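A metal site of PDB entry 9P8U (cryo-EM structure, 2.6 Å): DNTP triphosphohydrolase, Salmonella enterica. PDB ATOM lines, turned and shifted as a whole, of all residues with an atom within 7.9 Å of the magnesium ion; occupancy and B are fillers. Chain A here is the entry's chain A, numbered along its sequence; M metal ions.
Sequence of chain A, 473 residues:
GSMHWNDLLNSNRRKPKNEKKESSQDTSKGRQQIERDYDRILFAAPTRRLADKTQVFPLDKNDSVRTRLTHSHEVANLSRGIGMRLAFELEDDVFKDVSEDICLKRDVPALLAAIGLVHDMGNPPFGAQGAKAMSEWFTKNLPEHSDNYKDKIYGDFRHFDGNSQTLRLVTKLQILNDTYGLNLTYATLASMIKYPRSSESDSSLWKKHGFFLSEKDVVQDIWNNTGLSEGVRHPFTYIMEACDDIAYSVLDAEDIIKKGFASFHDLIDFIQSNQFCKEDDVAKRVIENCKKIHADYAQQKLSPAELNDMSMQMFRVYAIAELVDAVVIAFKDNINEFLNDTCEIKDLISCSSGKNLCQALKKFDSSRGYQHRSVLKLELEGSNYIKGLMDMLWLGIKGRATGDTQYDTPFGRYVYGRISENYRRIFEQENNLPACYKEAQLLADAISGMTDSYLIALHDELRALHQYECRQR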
ATOM      1  N   GLN A  55     -27.326 -25.684 -31.723  1.00  0.00           N
ATOM      2  CA  GLN A  55     -26.853 -26.867 -31.028  1.00  0.00           C
ATOM      3  C   GLN A  55     -27.031 -28.124 -31.867  1.00  0.00           C
ATOM      4  O   GLN A  55     -26.046 -28.816 -32.166  1.00  0.00           O
ATOM      5  CB  GLN A  55     -27.596 -27.013 -29.690  1.00  0.00           C
ATOM      6  CG  GLN A  55     -27.421 -28.363 -29.016  1.00  0.00           C
ATOM      7  CD  GLN A  55     -26.256 -28.388 -28.061  1.00  0.00           C
ATOM      8  OE1 GLN A  55     -25.662 -27.348 -27.755  1.00  0.00           O
ATOM      9  NE2 GLN A  55     -25.913 -29.577 -27.569  1.00  0.00           N
ATOM     10  N   ARG A  68     -27.169 -23.275 -27.991  1.00  0.00           N
ATOM     11  CA  ARG A  68     -26.002 -23.411 -27.127  1.00  0.00           C
ATOM     12  C   ARG A  68     -26.241 -22.750 -25.779  1.00  0.00           C
ATOM     13  O   ARG A  68     -25.826 -23.278 -24.745  1.00  0.00           O
ATOM     14  CB  ARG A  68     -24.771 -22.811 -27.811  1.00  0.00           C
ATOM     15  CG  ARG A  68     -24.369 -23.536 -29.085  1.00  0.00           C
ATOM     16  CD  ARG A  68     -23.410 -24.668 -28.789  1.00  0.00           C
ATOM     17  NE  ARG A  68     -22.764 -25.168 -30.002  1.00  0.00           N
ATOM     18  CZ  ARG A  68     -21.799 -24.525 -30.652  1.00  0.00           C
ATOM     19  NH1 ARG A  68     -21.336 -23.370 -30.235  1.00  0.00           N
ATOM     20  NH2 ARG A  68     -21.298 -25.066 -31.755  1.00  0.00           N
ATOM     21  N   HIS A  71     -28.788 -24.952 -23.735  1.00  0.00           N
ATOM     22  CA  HIS A  71     -28.126 -26.188 -23.321  1.00  0.00           C
ATOM     23  C   HIS A  71     -27.099 -25.907 -22.222  1.00  0.00           C
ATOM     24  O   HIS A  71     -26.998 -26.662 -21.251  1.00  0.00           O
ATOM     25  CB  HIS A  71     -27.459 -26.850 -24.526  1.00  0.00           C
ATOM     26  CG  HIS A  71     -26.405 -27.836 -24.170  1.00  0.00           C
ATOM     27  ND1 HIS A  71     -26.685 -29.118 -23.763  1.00  0.00           N
ATOM     28  CD2 HIS A  71     -25.046 -27.736 -24.182  1.00  0.00           C
ATOM     29  CE1 HIS A  71     -25.558 -29.769 -23.524  1.00  0.00           C
ATOM     30  NE2 HIS A  71     -24.555 -28.952 -23.768  1.00  0.00           N
ATOM     31  N   SER A  72     -26.344 -24.826 -22.363  1.00  0.00           N
ATOM     32  CA  SER A  72     -25.359 -24.464 -21.340  1.00  0.00           C
ATOM     33  C   SER A  72     -26.046 -24.152 -20.014  1.00  0.00           C
ATOM     34  O   SER A  72     -25.567 -24.552 -18.958  1.00  0.00           O
ATOM     35  CB  SER A  72     -24.520 -23.286 -21.810  1.00  0.00           C
ATOM     36  OG  SER A  72     -23.804 -23.608 -22.986  1.00  0.00           O
ATOM     37  N   VAL A  75     -27.196 -27.452 -18.444  1.00  0.00           N
ATOM     38  CA  VAL A  75     -26.065 -28.157 -17.871  1.00  0.00           C
ATOM     39  C   VAL A  75     -25.621 -27.485 -16.574  1.00  0.00           C
ATOM     40  O   VAL A  75     -25.306 -28.152 -15.588  1.00  0.00           O
ATOM     41  CB  VAL A  75     -24.915 -28.247 -18.890  1.00  0.00           C
ATOM     42  CG1 VAL A  75     -23.662 -28.814 -18.232  1.00  0.00           C
ATOM     43  CG2 VAL A  75     -25.314 -29.097 -20.070  1.00  0.00           C
ATOM     44  N   GLY A 116     -20.230 -25.713 -15.833  1.00  0.00           N
ATOM     45  CA  GLY A 116     -21.270 -26.167 -16.746  1.00  0.00           C
ATOM     46  C   GLY A 116     -21.666 -25.116 -17.751  1.00  0.00           C
ATOM     47  O   GLY A 116     -21.909 -25.427 -18.921  1.00  0.00           O
ATOM     48  N   HIS A 119     -18.878 -24.676 -20.519  1.00  0.00           N
ATOM     49  CA  HIS A 119     -18.322 -25.899 -21.076  1.00  0.00           C
ATOM     50  C   HIS A 119     -18.290 -25.899 -22.602  1.00  0.00           C
ATOM     51  O   HIS A 119     -17.449 -26.598 -23.189  1.00  0.00           O
ATOM     52  CB  HIS A 119     -19.101 -27.115 -20.573  1.00  0.00           C
ATOM     53  CG  HIS A 119     -20.288 -27.459 -21.423  1.00  0.00           C
ATOM     54  ND1 HIS A 119     -21.507 -26.820 -21.301  1.00  0.00           N
ATOM     55  CD2 HIS A 119     -20.449 -28.393 -22.396  1.00  0.00           C
ATOM     56  CE1 HIS A 119     -22.356 -27.335 -22.164  1.00  0.00           C
ATOM     57  NE2 HIS A 119     -21.747 -28.287 -22.841  1.00  0.00           N
ATOM     58  N   ASP A 120     -19.162 -25.144 -23.259  1.00  0.00           N
ATOM     59  CA  ASP A 120     -19.233 -25.115 -24.715  1.00  0.00           C
ATOM     60  C   ASP A 120     -19.142 -23.682 -25.225  1.00  0.00           C
ATOM     61  O   ASP A 120     -19.798 -23.301 -26.198  1.00  0.00           O
ATOM     62  CB  ASP A 120     -20.508 -25.776 -25.220  1.00  0.00           C
ATOM     63  CG  ASP A 120     -20.318 -27.265 -25.487  1.00  0.00           C
ATOM     64  OD1 ASP A 120     -19.160 -27.723 -25.481  1.00  0.00           O
ATOM     65  OD2 ASP A 120     -21.332 -27.966 -25.695  1.00  0.00           O
ATOM     66  N   ASN A 123     -16.832 -23.403 -28.801  1.00  0.00           N
ATOM     67  CA  ASN A 123     -17.051 -24.324 -29.912  1.00  0.00           C
ATOM     68  C   ASN A 123     -17.347 -23.531 -31.185  1.00  0.00           C
ATOM     69  O   ASN A 123     -17.977 -22.471 -31.135  1.00  0.00           O
ATOM     70  CB  ASN A 123     -18.207 -25.270 -29.605  1.00  0.00           C
ATOM     71  CG  ASN A 123     -17.895 -26.213 -28.473  1.00  0.00           C
ATOM     72  OD1 ASN A 123     -16.874 -26.076 -27.791  1.00  0.00           O
ATOM     73  ND2 ASN A 123     -18.763 -27.189 -28.259  1.00  0.00           N
ATOM     74  N   ASN A 163     -13.049 -27.745 -26.925  1.00  0.00           N
ATOM     75  CA  ASN A 163     -12.628 -27.530 -25.540  1.00  0.00           C
ATOM     76  C   ASN A 163     -11.348 -26.711 -25.463  1.00  0.00           C
ATOM     77  O   ASN A 163     -11.228 -25.818 -24.607  1.00  0.00           O
ATOM     78  CB  ASN A 163     -12.447 -28.884 -24.845  1.00  0.00           C
ATOM     79  CG  ASN A 163     -13.692 -29.740 -24.903  1.00  0.00           C
ATOM     80  OD1 ASN A 163     -13.691 -30.813 -25.493  1.00  0.00           O
ATOM     81  ND2 ASN A 163     -14.766 -29.250 -24.284  1.00  0.00           N
ATOM     82  N   LYS A 194     -11.419 -30.611 -19.885  1.00  0.00           N
ATOM     83  CA  LYS A 194     -12.055 -31.917 -20.077  1.00  0.00           C
ATOM     84  C   LYS A 194     -11.023 -33.004 -20.304  1.00  0.00           C
ATOM     85  O   LYS A 194     -11.110 -34.096 -19.724  1.00  0.00           O
ATOM     86  CB  LYS A 194     -13.039 -31.855 -21.248  1.00  0.00           C
ATOM     87  CG  LYS A 194     -14.491 -31.956 -20.854  1.00  0.00           C
ATOM     88  CD  LYS A 194     -15.363 -32.240 -22.077  1.00  0.00           C
ATOM     89  CE  LYS A 194     -16.820 -32.422 -21.690  1.00  0.00           C
ATOM     90  NZ  LYS A 194     -17.415 -31.165 -21.162  1.00  0.00           N
ATOM     91  N   MET A 240     -19.282 -32.423 -14.395  1.00  0.00           N
ATOM     92  CA  MET A 240     -19.708 -31.543 -15.469  1.00  0.00           C
ATOM     93  C   MET A 240     -19.950 -32.324 -16.762  1.00  0.00           C
ATOM     94  O   MET A 240     -20.937 -32.076 -17.456  1.00  0.00           O
ATOM     95  CB  MET A 240     -18.676 -30.444 -15.702  1.00  0.00           C
ATOM     96  CG  MET A 240     -19.065 -29.453 -16.782  1.00  0.00           C
ATOM     97  SD  MET A 240     -18.226 -29.752 -18.349  1.00  0.00           S
ATOM     98  CE  MET A 240     -16.523 -29.882 -17.800  1.00  0.00           C
ATOM     99  N   GLU A 241     -19.054 -33.249 -17.084  1.00  0.00           N
ATOM    100  CA  GLU A 241     -19.225 -34.056 -18.286  1.00  0.00           C
ATOM    101  C   GLU A 241     -20.455 -34.944 -18.204  1.00  0.00           C
ATOM    102  O   GLU A 241     -21.186 -35.095 -19.190  1.00  0.00           O
ATOM    103  CB  GLU A 241     -17.971 -34.890 -18.533  1.00  0.00           C
ATOM    104  CG  GLU A 241     -18.134 -36.009 -19.536  1.00  0.00           C
ATOM    105  CD  GLU A 241     -17.100 -37.097 -19.366  1.00  0.00           C
ATOM    106  OE1 GLU A 241     -17.016 -37.672 -18.264  1.00  0.00           O
ATOM    107  OE2 GLU A 241     -16.376 -37.400 -20.347  1.00  0.00           O
ATOM    108  N   CYS A 243     -23.169 -34.330 -16.431  1.00  0.00           N
ATOM    109  CA  CYS A 243     -24.332 -33.456 -16.556  1.00  0.00           C
ATOM    110  C   CYS A 243     -24.543 -33.036 -18.009  1.00  0.00           C
ATOM    111  O   CYS A 243     -25.680 -33.008 -18.488  1.00  0.00           O
ATOM    112  CB  CYS A 243     -24.163 -32.221 -15.672  1.00  0.00           C
ATOM    113  SG  CYS A 243     -24.451 -32.530 -13.924  1.00  0.00           S
ATOM    114  N   ASP A 244     -23.454 -32.734 -18.717  1.00  0.00           N
ATOM    115  CA  ASP A 244     -23.569 -32.375 -20.135  1.00  0.00           C
ATOM    116  C   ASP A 244     -24.127 -33.541 -20.940  1.00  0.00           C
ATOM    117  O   ASP A 244     -25.005 -33.347 -21.801  1.00  0.00           O
ATOM    118  CB  ASP A 244     -22.203 -31.947 -20.675  1.00  0.00           C
ATOM    119  CG  ASP A 244     -22.224 -31.644 -22.150  1.00  0.00           C
ATOM    120  OD1 ASP A 244     -22.852 -30.642 -22.549  1.00  0.00           O
ATOM    121  OD2 ASP A 244     -21.612 -32.401 -22.925  1.00  0.00           O
ATOM    122  N   ASP A 245     -23.643 -34.752 -20.672  1.00  0.00           N
ATOM    123  CA  ASP A 245     -24.136 -35.931 -21.387  1.00  0.00           C
ATOM    124  C   ASP A 245     -25.620 -36.141 -21.127  1.00  0.00           C
ATOM    125  O   ASP A 245     -26.395 -36.347 -22.064  1.00  0.00           O
ATOM    126  CB  ASP A 245     -23.325 -37.161 -20.983  1.00  0.00           C
ATOM    127  CG  ASP A 245     -21.937 -37.176 -21.573  1.00  0.00           C
ATOM    128  OD1 ASP A 245     -21.615 -36.245 -22.342  1.00  0.00           O
ATOM    129  OD2 ASP A 245     -21.174 -38.118 -21.275  1.00  0.00           O
ATOM    130  N   ALA A 247     -27.873 -33.997 -20.068  1.00  0.00           N
ATOM    131  CA  ALA A 247     -28.673 -32.904 -20.614  1.00  0.00           C
ATOM    132  C   ALA A 247     -28.838 -33.051 -22.121  1.00  0.00           C
ATOM    133  O   ALA A 247     -29.966 -33.006 -22.632  1.00  0.00           O
ATOM    134  CB  ALA A 247     -28.032 -31.562 -20.266  1.00  0.00           C
ATOM    135  N   TYR A 248     -27.739 -33.242 -22.847  1.00  0.00           N
ATOM    136  CA  TYR A 248     -27.859 -33.298 -24.300  1.00  0.00           C
ATOM    137  C   TYR A 248     -28.636 -34.540 -24.724  1.00  0.00           C
ATOM    138  O   TYR A 248     -29.521 -34.466 -25.577  1.00  0.00           O
ATOM    139  CB  TYR A 248     -26.478 -33.213 -24.953  1.00  0.00           C
ATOM    140  CG  TYR A 248     -25.797 -34.510 -25.358  1.00  0.00           C
ATOM    141  CD1 TYR A 248     -26.194 -35.205 -26.498  1.00  0.00           C
ATOM    142  CD2 TYR A 248     -24.731 -35.008 -24.629  1.00  0.00           C
ATOM    143  CE1 TYR A 248     -25.570 -36.368 -26.875  1.00  0.00           C
ATOM    144  CE2 TYR A 248     -24.103 -36.168 -24.998  1.00  0.00           C
ATOM    145  CZ  TYR A 248     -24.523 -36.848 -26.121  1.00  0.00           C
ATOM    146  OH  TYR A 248     -23.886 -38.012 -26.493  1.00  0.00           O
HETATM  147 MG    MG M   1     -22.533 -29.641 -24.214  1.00  0.00          MG
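Four residues have an atom within 4 Å of the magnesium ion: His 71, His 119, Asp 120 and Asp 244.
A ring nitrogen (ND1) of His 119 lies within hydrogen-bond range of the backbone carbonyl oxygen (O) of Gly 116, at 2.8 Å.
The side-chain carboxylate (OD1) of Asp 120 is in hydrogen-bond range of the side-chain amide nitrogen (ND2) of Asn 123.
The magnesium ion is bound by the side-chain carboxylate of Asp 244 (2.0 Å), a ring nitrogen (NE2) of His 119 (2.1 Å), a ring nitrogen (NE2) of His 71 (2.2 Å) and the side-chain carboxylate of Asp 120 (2.5 Å).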
